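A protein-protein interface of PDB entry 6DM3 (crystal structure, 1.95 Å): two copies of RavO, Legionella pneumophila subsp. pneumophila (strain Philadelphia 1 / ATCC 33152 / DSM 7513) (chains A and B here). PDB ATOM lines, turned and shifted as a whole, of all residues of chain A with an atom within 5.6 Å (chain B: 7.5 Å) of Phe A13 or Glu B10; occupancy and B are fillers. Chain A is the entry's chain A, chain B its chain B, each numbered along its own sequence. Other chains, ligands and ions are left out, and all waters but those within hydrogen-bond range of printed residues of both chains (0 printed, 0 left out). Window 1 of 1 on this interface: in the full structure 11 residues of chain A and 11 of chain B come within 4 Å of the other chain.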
ATOM      1  N   VAL A   8     -16.634   7.136  -6.701  1.00  0.00           N
ATOM      2  CA  VAL A   8     -15.578   8.139  -6.604  1.00  0.00           C
ATOM      3  C   VAL A   8     -14.777   7.961  -5.301  1.00  0.00           C
ATOM      4  O   VAL A   8     -13.556   8.113  -5.296  1.00  0.00           O
ATOM      5  CB  VAL A   8     -16.139   9.580  -6.676  1.00  0.00           C
ATOM      6  CG1 VAL A   8     -15.057  10.590  -6.334  1.00  0.00           C
ATOM      7  CG2 VAL A   8     -16.706   9.874  -8.061  1.00  0.00           C
ATOM      8  N   MET A   9     -15.452   7.621  -4.202  1.00  0.00           N
ATOM      9  CA  MET A   9     -14.775   7.456  -2.910  1.00  0.00           C
ATOM     10  C   MET A   9     -13.946   6.170  -2.864  1.00  0.00           C
ATOM     11  O   MET A   9     -12.938   6.091  -2.153  1.00  0.00           O
ATOM     12  CB  MET A   9     -15.789   7.463  -1.768  1.00  0.00           C
ATOM     13  CG  MET A   9     -16.502   8.798  -1.588  1.00  0.00           C
ATOM     14  SD  MET A   9     -17.693   8.750  -0.239  1.00  0.00           S
ATOM     15  CE  MET A   9     -18.592   7.262  -0.666  1.00  0.00           C
ATOM     16  N   GLU A  10     -14.375   5.161  -3.619  1.00  0.00           N
ATOM     17  CA  GLU A  10     -13.595   3.934  -3.766  1.00  0.00           C
ATOM     18  C   GLU A  10     -12.216   4.245  -4.346  1.00  0.00           C
ATOM     19  O   GLU A  10     -11.206   3.784  -3.817  1.00  0.00           O
ATOM     20  CB  GLU A  10     -14.320   2.925  -4.659  1.00  0.00           C
ATOM     21  CG  GLU A  10     -13.516   1.644  -4.930  1.00  0.00           C
ATOM     22  CD  GLU A  10     -14.144   0.760  -6.000  1.00  0.00           C
ATOM     23  OE1 GLU A  10     -15.027  -0.060  -5.667  1.00  0.00           O
ATOM     24  OE2 GLU A  10     -13.746   0.879  -7.177  1.00  0.00           O
ATOM     25  N   GLU A  11     -12.170   5.039  -5.419  1.00  0.00           N
ATOM     26  CA  GLU A  11     -10.900   5.421  -6.047  1.00  0.00           C
ATOM     27  C   GLU A  11      -9.953   6.111  -5.067  1.00  0.00           C
ATOM     28  O   GLU A  11      -8.735   5.923  -5.126  1.00  0.00           O
ATOM     29  CB  GLU A  11     -11.142   6.348  -7.242  1.00  0.00           C
ATOM     30  CG  GLU A  11     -11.813   5.687  -8.436  1.00  0.00           C
ATOM     31  CD  GLU A  11     -11.679   6.516  -9.700  1.00  0.00           C
ATOM     32  OE1 GLU A  11     -10.664   7.228  -9.832  1.00  0.00           O
ATOM     33  OE2 GLU A  11     -12.585   6.455 -10.560  1.00  0.00           O
ATOM     34  N   ILE A  12     -10.525   6.911  -4.172  1.00  0.00           N
ATOM     35  CA  ILE A  12      -9.756   7.659  -3.181  1.00  0.00           C
ATOM     36  C   ILE A  12      -9.286   6.781  -2.028  1.00  0.00           C
ATOM     37  O   ILE A  12      -8.095   6.733  -1.719  1.00  0.00           O
ATOM     38  CB  ILE A  12     -10.578   8.825  -2.611  1.00  0.00           C
ATOM     39  CG1 ILE A  12     -10.944   9.814  -3.721  1.00  0.00           C
ATOM     40  CG2 ILE A  12      -9.802   9.540  -1.495  1.00  0.00           C
ATOM     41  CD1 ILE A  12     -11.726  11.006  -3.235  1.00  0.00           C
ATOM     42  N   PHE A  13     -10.228   6.076  -1.404  1.00  0.00           N
ATOM     43  CA  PHE A  13      -9.949   5.312  -0.186  1.00  0.00           C
ATOM     44  C   PHE A  13      -9.025   4.104  -0.403  1.00  0.00           C
ATOM     45  O   PHE A  13      -8.315   3.695   0.517  1.00  0.00           O
ATOM     46  CB  PHE A  13     -11.271   4.867   0.462  1.00  0.00           C
ATOM     47  CG  PHE A  13     -12.067   6.004   1.044  1.00  0.00           C
ATOM     48  CD1 PHE A  13     -11.439   7.194   1.374  1.00  0.00           C
ATOM     49  CD2 PHE A  13     -13.430   5.885   1.268  1.00  0.00           C
ATOM     50  CE1 PHE A  13     -12.151   8.244   1.908  1.00  0.00           C
ATOM     51  CE2 PHE A  13     -14.152   6.939   1.808  1.00  0.00           C
ATOM     52  CZ  PHE A  13     -13.507   8.119   2.127  1.00  0.00           C
ATOM     53  N   VAL A  14      -9.026   3.531  -1.604  1.00  0.00           N
ATOM     54  CA  VAL A  14      -8.166   2.379  -1.874  1.00  0.00           C
ATOM     55  C   VAL A  14      -6.740   2.821  -2.191  1.00  0.00           C
ATOM     56  O   VAL A  14      -5.804   2.012  -2.150  1.00  0.00           O
ATOM     57  CB  VAL A  14      -8.682   1.501  -3.056  1.00  0.00           C
ATOM     58  CG1 VAL A  14     -10.114   1.060  -2.823  1.00  0.00           C
ATOM     59  CG2 VAL A  14      -8.545   2.221  -4.387  1.00  0.00           C
ATOM     60  N   ASP A  15      -6.572   4.100  -2.510  1.00  0.00           N
ATOM     61  CA  ASP A  15      -5.278   4.596  -2.959  1.00  0.00           C
ATOM     62  C   ASP A  15      -4.266   4.615  -1.823  1.00  0.00           C
ATOM     63  O   ASP A  15      -4.612   4.873  -0.665  1.00  0.00           O
ATOM     64  CB  ASP A  15      -5.413   5.998  -3.562  1.00  0.00           C
ATOM     65  CG  ASP A  15      -4.125   6.480  -4.211  1.00  0.00           C
ATOM     66  OD1 ASP A  15      -3.272   7.037  -3.490  1.00  0.00           O
ATOM     67  OD2 ASP A  15      -3.969   6.308  -5.441  1.00  0.00           O
ATOM     68  N   TYR A  18      -4.085   7.628   0.538  1.00  0.00           N
ATOM     69  CA  TYR A  18      -5.101   7.807   1.571  1.00  0.00           C
ATOM     70  C   TYR A  18      -4.616   7.207   2.885  1.00  0.00           C
ATOM     71  O   TYR A  18      -4.179   6.053   2.938  1.00  0.00           O
ATOM     72  CB  TYR A  18      -6.450   7.183   1.174  1.00  0.00           C
ATOM     73  CG  TYR A  18      -7.545   7.581   2.142  1.00  0.00           C
ATOM     74  CD1 TYR A  18      -8.126   8.848   2.068  1.00  0.00           C
ATOM     75  CD2 TYR A  18      -7.960   6.720   3.157  1.00  0.00           C
ATOM     76  CE1 TYR A  18      -9.102   9.237   2.967  1.00  0.00           C
ATOM     77  CE2 TYR A  18      -8.939   7.103   4.058  1.00  0.00           C
ATOM     78  CZ  TYR A  18      -9.505   8.362   3.959  1.00  0.00           C
ATOM     79  OH  TYR A  18     -10.481   8.751   4.852  1.00  0.00           O
ATOM     80  N   GLU A  20      -5.903   6.400   6.468  1.00  0.00           N
ATOM     81  CA  GLU A  20      -7.073   6.263   7.335  1.00  0.00           C
ATOM     82  C   GLU A  20      -6.716   6.392   8.815  1.00  0.00           C
ATOM     83  O   GLU A  20      -7.598   6.522   9.660  1.00  0.00           O
ATOM     84  CB  GLU A  20      -7.776   4.923   7.077  1.00  0.00           C
ATOM     85  CG  GLU A  20      -7.003   3.683   7.503  1.00  0.00           C
ATOM     86  CD  GLU A  20      -6.089   3.153   6.413  1.00  0.00           C
ATOM     87  OE1 GLU A  20      -5.976   3.809   5.352  1.00  0.00           O
ATOM     88  OE2 GLU A  20      -5.481   2.079   6.618  1.00  0.00           O
ATOM     89  N   ARG A  23      -5.674  11.327  11.684  1.00  0.00           N
ATOM     90  CA  ARG A  23      -6.920  12.027  11.965  1.00  0.00           C
ATOM     91  C   ARG A  23      -6.745  13.388  12.641  1.00  0.00           C
ATOM     92  O   ARG A  23      -7.728  14.091  12.870  1.00  0.00           O
ATOM     93  CB  ARG A  23      -7.825  11.152  12.835  1.00  0.00           C
ATOM     94  CG  ARG A  23      -8.313   9.881  12.157  1.00  0.00           C
ATOM     95  CD  ARG A  23      -9.206  10.233  10.976  1.00  0.00           C
ATOM     96  NE  ARG A  23      -9.707   9.058  10.267  1.00  0.00           N
ATOM     97  CZ  ARG A  23      -9.520   8.822   8.970  1.00  0.00           C
ATOM     98  NH1 ARG A  23      -8.798   9.656   8.232  1.00  0.00           N
ATOM     99  NH2 ARG A  23     -10.029   7.730   8.416  1.00  0.00           N
ATOM    100  N   TRP A  43      -9.449  11.736   5.798  1.00  0.00           N
ATOM    101  CA  TRP A  43     -10.822  12.068   6.127  1.00  0.00           C
ATOM    102  C   TRP A  43     -10.870  13.409   6.857  1.00  0.00           C
ATOM    103  O   TRP A  43     -10.233  13.579   7.900  1.00  0.00           O
ATOM    104  CB  TRP A  43     -11.398  10.940   6.981  1.00  0.00           C
ATOM    105  CG  TRP A  43     -12.840  11.039   7.316  1.00  0.00           C
ATOM    106  CD1 TRP A  43     -13.387  11.586   8.439  1.00  0.00           C
ATOM    107  CD2 TRP A  43     -13.929  10.540   6.538  1.00  0.00           C
ATOM    108  NE1 TRP A  43     -14.761  11.472   8.400  1.00  0.00           N
ATOM    109  CE2 TRP A  43     -15.115  10.835   7.243  1.00  0.00           C
ATOM    110  CE3 TRP A  43     -14.017   9.881   5.309  1.00  0.00           C
ATOM    111  CZ2 TRP A  43     -16.370  10.493   6.757  1.00  0.00           C
ATOM    112  CZ3 TRP A  43     -15.266   9.542   4.828  1.00  0.00           C
ATOM    113  CH2 TRP A  43     -16.425   9.848   5.552  1.00  0.00           C
ATOM    114  N   VAL A  56     -19.037  14.906   0.866  1.00  0.00           N
ATOM    115  CA  VAL A  56     -18.063  14.144   1.628  1.00  0.00           C
ATOM    116  C   VAL A  56     -16.736  14.878   1.492  1.00  0.00           C
ATOM    117  O   VAL A  56     -16.266  15.128   0.378  1.00  0.00           O
ATOM    118  CB  VAL A  56     -17.933  12.693   1.141  1.00  0.00           C
ATOM    119  CG1 VAL A  56     -16.715  12.037   1.765  1.00  0.00           C
ATOM    120  CG2 VAL A  56     -19.189  11.915   1.487  1.00  0.00           C
ATOM    121  N   ILE A  58     -12.764  15.488   1.808  1.00  0.00           N
ATOM    122  CA  ILE A  58     -11.438  14.896   1.860  1.00  0.00           C
ATOM    123  C   ILE A  58     -10.380  15.993   1.978  1.00  0.00           C
ATOM    124  O   ILE A  58     -10.442  17.006   1.280  1.00  0.00           O
ATOM    125  CB  ILE A  58     -11.162  14.033   0.614  1.00  0.00           C
ATOM    126  CG1 ILE A  58     -12.237  12.955   0.470  1.00  0.00           C
ATOM    127  CG2 ILE A  58      -9.775  13.422   0.678  1.00  0.00           C
ATOM    128  CD1 ILE A  58     -12.289  12.005   1.638  1.00  0.00           C
ATOM    129  N   LYS B   4     -22.995   8.134   8.279  1.00  0.00           N
ATOM    130  CA  LYS B   4     -22.279   6.949   8.746  1.00  0.00           C
ATOM    131  C   LYS B   4     -21.913   5.935   7.663  1.00  0.00           C
ATOM    132  O   LYS B   4     -20.973   5.158   7.831  1.00  0.00           O
ATOM    133  CB  LYS B   4     -23.074   6.254   9.856  1.00  0.00           C
ATOM    134  CG  LYS B   4     -22.223   5.430  10.808  1.00  0.00           C
ATOM    135  CD  LYS B   4     -21.638   6.294  11.913  1.00  0.00           C
ATOM    136  CE  LYS B   4     -20.789   5.470  12.867  1.00  0.00           C
ATOM    137  NZ  LYS B   4     -21.546   4.318  13.430  1.00  0.00           N
ATOM    138  N   ILE B   5     -22.649   5.937   6.557  1.00  0.00           N
ATOM    139  CA  ILE B   5     -22.380   4.984   5.479  1.00  0.00           C
ATOM    140  C   ILE B   5     -21.059   5.300   4.771  1.00  0.00           C
ATOM    141  O   ILE B   5     -20.339   4.393   4.360  1.00  0.00           O
ATOM    142  CB  ILE B   5     -23.540   4.940   4.442  1.00  0.00           C
ATOM    143  CG1 ILE B   5     -23.224   3.934   3.326  1.00  0.00           C
ATOM    144  CG2 ILE B   5     -23.839   6.330   3.891  1.00  0.00           C
ATOM    145  CD1 ILE B   5     -24.302   3.796   2.278  1.00  0.00           C
ATOM    146  N   TYR B   6     -20.727   6.583   4.654  1.00  0.00           N
ATOM    147  CA  TYR B   6     -19.491   6.986   3.990  1.00  0.00           C
ATOM    148  C   TYR B   6     -18.273   6.525   4.804  1.00  0.00           C
ATOM    149  O   TYR B   6     -17.224   6.192   4.244  1.00  0.00           O
ATOM    150  CB  TYR B   6     -19.471   8.503   3.768  1.00  0.00           C
ATOM    151  CG  TYR B   6     -20.639   9.014   2.940  1.00  0.00           C
ATOM    152  CD1 TYR B   6     -20.744   8.696   1.587  1.00  0.00           C
ATOM    153  CD2 TYR B   6     -21.628   9.819   3.502  1.00  0.00           C
ATOM    154  CE1 TYR B   6     -21.800   9.154   0.823  1.00  0.00           C
ATOM    155  CE2 TYR B   6     -22.689  10.283   2.742  1.00  0.00           C
ATOM    156  CZ  TYR B   6     -22.767   9.947   1.404  1.00  0.00           C
ATOM    157  OH  TYR B   6     -23.820  10.406   0.643  1.00  0.00           O
ATOM    158  N   LYS B   7     -18.436   6.477   6.125  1.00  0.00           N
ATOM    159  CA  LYS B   7     -17.379   6.012   7.024  1.00  0.00           C
ATOM    160  C   LYS B   7     -17.279   4.485   7.068  1.00  0.00           C
ATOM    161  O   LYS B   7     -16.191   3.940   7.252  1.00  0.00           O
ATOM    162  CB  LYS B   7     -17.605   6.554   8.437  1.00  0.00           C
ATOM    163  CG  LYS B   7     -16.692   7.712   8.837  1.00  0.00           C
ATOM    164  CD  LYS B   7     -15.228   7.284   8.901  1.00  0.00           C
ATOM    165  CE  LYS B   7     -14.351   8.350   9.556  1.00  0.00           C
ATOM    166  NZ  LYS B   7     -12.898   7.987   9.598  1.00  0.00           N
ATOM    167  N   VAL B   8     -18.412   3.800   6.918  1.00  0.00           N
ATOM    168  CA  VAL B   8     -18.422   2.339   6.819  1.00  0.00           C
ATOM    169  C   VAL B   8     -17.710   1.901   5.538  1.00  0.00           C
ATOM    170  O   VAL B   8     -16.898   0.969   5.552  1.00  0.00           O
ATOM    171  CB  VAL B   8     -19.862   1.758   6.837  1.00  0.00           C
ATOM    172  CG1 VAL B   8     -19.830   0.259   6.561  1.00  0.00           C
ATOM    173  CG2 VAL B   8     -20.546   2.029   8.168  1.00  0.00           C
ATOM    174  N   MET B   9     -18.018   2.585   4.436  1.00  0.00           N
ATOM    175  CA  MET B   9     -17.379   2.335   3.143  1.00  0.00           C
ATOM    176  C   MET B   9     -15.882   2.537   3.252  1.00  0.00           C
ATOM    177  O   MET B   9     -15.091   1.771   2.700  1.00  0.00           O
ATOM    178  CB  MET B   9     -17.933   3.263   2.058  1.00  0.00           C
ATOM    179  CG  MET B   9     -19.373   3.002   1.712  1.00  0.00           C
ATOM    180  SD  MET B   9     -19.591   1.245   1.397  1.00  0.00           S
ATOM    181  CE  MET B   9     -21.309   1.039   1.826  1.00  0.00           C
ATOM    182  N   GLU B  10     -15.504   3.590   3.965  1.00  0.00           N
ATOM    183  CA  GLU B  10     -14.105   3.902   4.186  1.00  0.00           C
ATOM    184  C   GLU B  10     -13.408   2.743   4.901  1.00  0.00           C
ATOM    185  O   GLU B  10     -12.329   2.330   4.497  1.00  0.00           O
ATOM    186  CB  GLU B  10     -13.961   5.191   4.997  1.00  0.00           C
ATOM    187  CG  GLU B  10     -12.535   5.745   5.008  1.00  0.00           C
ATOM    188  CD  GLU B  10     -11.921   5.756   6.394  1.00  0.00           C
ATOM    189  OE1 GLU B  10     -10.906   6.456   6.600  1.00  0.00           O
ATOM    190  OE2 GLU B  10     -12.463   5.065   7.281  1.00  0.00           O
ATOM    191  N   GLU B  11     -14.027   2.207   5.950  1.00  0.00           N
ATOM    192  CA  GLU B  11     -13.448   1.061   6.658  1.00  0.00           C
ATOM    193  C   GLU B  11     -13.313  -0.147   5.734  1.00  0.00           C
ATOM    194  O   GLU B  11     -12.349  -0.916   5.825  1.00  0.00           O
ATOM    195  CB  GLU B  11     -14.298   0.684   7.864  1.00  0.00           C
ATOM    196  CG  GLU B  11     -14.377   1.766   8.928  1.00  0.00           C
ATOM    197  CD  GLU B  11     -14.887   1.233  10.248  1.00  0.00           C
ATOM    198  OE1 GLU B  11     -14.672   0.034  10.515  1.00  0.00           O
ATOM    199  OE2 GLU B  11     -15.488   2.008  11.022  1.00  0.00           O
ATOM    200  N   ILE B  12     -14.280  -0.307   4.833  1.00  0.00           N
ATOM    201  CA  ILE B  12     -14.266  -1.414   3.878  1.00  0.00           C
ATOM    202  C   ILE B  12     -13.249  -1.204   2.748  1.00  0.00           C
ATOM    203  O   ILE B  12     -12.445  -2.093   2.460  1.00  0.00           O
ATOM    204  CB  ILE B  12     -15.669  -1.642   3.267  1.00  0.00           C
ATOM    205  CG1 ILE B  12     -16.647  -2.121   4.351  1.00  0.00           C
ATOM    206  CG2 ILE B  12     -15.600  -2.661   2.124  1.00  0.00           C
ATOM    207  CD1 ILE B  12     -18.008  -2.542   3.832  1.00  0.00           C
ATOM    208  N   PHE B  13     -13.268  -0.031   2.120  1.00  0.00           N
ATOM    209  CA  PHE B  13     -12.450   0.203   0.921  1.00  0.00           C
ATOM    210  C   PHE B  13     -10.939   0.311   1.209  1.00  0.00           C
ATOM    211  O   PHE B  13     -10.115   0.051   0.325  1.00  0.00           O
ATOM    212  CB  PHE B  13     -12.936   1.462   0.185  1.00  0.00           C
ATOM    213  CG  PHE B  13     -14.274   1.295  -0.500  1.00  0.00           C
ATOM    214  CD1 PHE B  13     -14.748   0.032  -0.815  1.00  0.00           C
ATOM    215  CD2 PHE B  13     -15.052   2.399  -0.825  1.00  0.00           C
ATOM    216  CE1 PHE B  13     -15.972  -0.131  -1.439  1.00  0.00           C
ATOM    217  CE2 PHE B  13     -16.279   2.241  -1.452  1.00  0.00           C
ATOM    218  CZ  PHE B  13     -16.738   0.978  -1.760  1.00  0.00           C
ATOM    219  N   VAL B  14     -10.574   0.682   2.438  1.00  0.00           N
ATOM    220  CA  VAL B  14      -9.164   0.782   2.821  1.00  0.00           C
ATOM    221  C   VAL B  14      -8.589  -0.580   3.198  1.00  0.00           C
ATOM    222  O   VAL B  14      -7.375  -0.720   3.379  1.00  0.00           O
ATOM    223  CB  VAL B  14      -8.930   1.742   4.024  1.00  0.00           C
ATOM    224  CG1 VAL B  14      -9.444   3.147   3.726  1.00  0.00           C
ATOM    225  CG2 VAL B  14      -9.546   1.186   5.301  1.00  0.00           C
ATOM    226  N   ASP B  15      -9.445  -1.589   3.329  1.00  0.00           N
ATOM    227  CA  ASP B  15      -8.972  -2.865   3.853  1.00  0.00           C
ATOM    228  C   ASP B  15      -8.217  -3.680   2.813  1.00  0.00           C
ATOM    229  O   ASP B  15      -8.501  -3.631   1.612  1.00  0.00           O
ATOM    230  CB  ASP B  15     -10.121  -3.703   4.412  1.00  0.00           C
ATOM    231  CG  ASP B  15      -9.626  -4.963   5.115  1.00  0.00           C
ATOM    232  OD1 ASP B  15      -9.240  -4.863   6.301  1.00  0.00           O
ATOM    233  OD2 ASP B  15      -9.621  -6.047   4.487  1.00  0.00           O
ATOM    234  N   TYR B  18     -10.249  -5.830   0.299  1.00  0.00           N
ATOM    235  CA  TYR B  18     -11.062  -5.217  -0.752  1.00  0.00           C
ATOM    236  C   TYR B  18     -10.296  -5.178  -2.079  1.00  0.00           C
ATOM    237  O   TYR B  18      -9.172  -4.667  -2.157  1.00  0.00           O
ATOM    238  CB  TYR B  18     -11.528  -3.804  -0.373  1.00  0.00           C
ATOM    239  CG  TYR B  18     -12.517  -3.254  -1.384  1.00  0.00           C
ATOM    240  CD1 TYR B  18     -13.858  -3.639  -1.350  1.00  0.00           C
ATOM    241  CD2 TYR B  18     -12.098  -2.401  -2.403  1.00  0.00           C
ATOM    242  CE1 TYR B  18     -14.753  -3.168  -2.282  1.00  0.00           C
ATOM    243  CE2 TYR B  18     -12.992  -1.925  -3.340  1.00  0.00           C
ATOM    244  CZ  TYR B  18     -14.317  -2.315  -3.273  1.00  0.00           C
ATOM    245  OH  TYR B  18     -15.212  -1.841  -4.202  1.00  0.00           O
ATOM    246  N   MET B 102     -14.305  -4.284   9.745  1.00  0.00           N
ATOM    247  CA  MET B 102     -13.503  -5.324   9.122  1.00  0.00           C
ATOM    248  C   MET B 102     -13.306  -6.484  10.083  1.00  0.00           C
ATOM    249  O   MET B 102     -13.349  -7.630   9.670  1.00  0.00           O
ATOM    250  CB  MET B 102     -12.155  -4.783   8.639  1.00  0.00           C
ATOM    251  CG  MET B 102     -12.224  -4.082   7.284  1.00  0.00           C
ATOM    252  SD  MET B 102     -13.243  -4.933   6.044  1.00  0.00           S
ATOM    253  CE  MET B 102     -12.502  -6.569   5.996  1.00  0.00           C
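Glu B10 touches four residues of chain A.
Printed residues of chain A within 4 Å of Val B14: Phe A13 (3.4 Å), Tyr A18 (3.9 Å) and Glu A20 (3.8 Å).
Printed residues of chain A within 4 Å of Tyr B18: Glu A10 (2.3 Å).
Printed residues of chain A within 4 Å of Lys B7: Arg A23 and Trp A43.
Of the printed residues of chain A, Phe B13 touches Glu A10, Phe A13 and Val A14.
Lys B4 touches none of the printed residues of chain A.
The nearest printed residue of chain B that does not touch Phe A13 is Met B9 (4.6 Å).
The nearest printed residue of chain B that does not touch Glu A20 is Lys B7 (5.5 Å).
Printed residues of chain B that touch a printed residue of chain A: Tyr B6, Lys B7, Glu B10, Phe B13, Val B14 and Tyr B18.
Hydrophobic or aromatic side chains of chain B that line the printed part of chain A: Tyr B6, Phe B13, Val B14 and Tyr B18.
Hydrophobic or aromatic side chains of chain A within 4 Å of the printed part of chain B: Met A9, Phe A13, Val A14, Tyr A18, Trp A43 and Val A56.
Along chain A the printed residues that touch a printed residue of chain B span positions 9 to 56.
Among the printed residues, Asp or Glu carboxylates within 4 Å of a Lys or Arg side-chain nitrogen of the other chain: Arg A23 with Glu B10.
The side-chain hydroxyl (OH) of Tyr A18 sits close to the backbone NH (N) of Trp A43, at 3.3 Å.
The guanidinium group (NH2) of Arg A23 lies within hydrogen-bond range of the backbone carbonyl oxygen (O) of Glu A20 (3.0 Å).
OE2 of Glu B10 lies within salt-bridge range of NZ of Lys B7, 3.8 Å away.
Phe B13 touches Glu A10.
CE2 of Phe A13 touches O of Tyr B6, at 3.99 Å.
Phe A13 touches Glu B10.
Val B14 touches Phe A13.
O of Phe B13 touches CG1 of Val A14, at 3.3 Å.
Tyr A18 touches Val B14 (CD2 to CG1, 3.9 Å).
Glu A20 touches Glu B10.
OE1 of Glu A20 touches CB of Val B14, at 3.8 Å.
Trp A43 touches Lys B7.
Val A56 touches Tyr B6.
Glu A10 touches Phe B13, and with the chains exchanged Phe A13 touches Glu B10.
Glu A10 touches Tyr B18, and with the chains exchanged Tyr A18 touches Glu B10.
Phe A13 touches its own counterpart, Phe B13.
Phe A13 touches Val B14, and with the chains exchanged Val A14 touches Phe B13.
OH of Tyr A18 lies within hydrogen-bond range of OE1 of Glu B10, 2.9 Å away.
NH2 of Arg A23 is in salt-bridge range of OE2 of Glu B10, 3.8 Å away.
The side-chain hydroxyl (OH) of Tyr B18 sits close to the side-chain carboxylate (OE1) of Glu A10 (2.3 Å).
NH2 of Arg A23 lies close to NZ of Lys B7 (3.1 Å).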
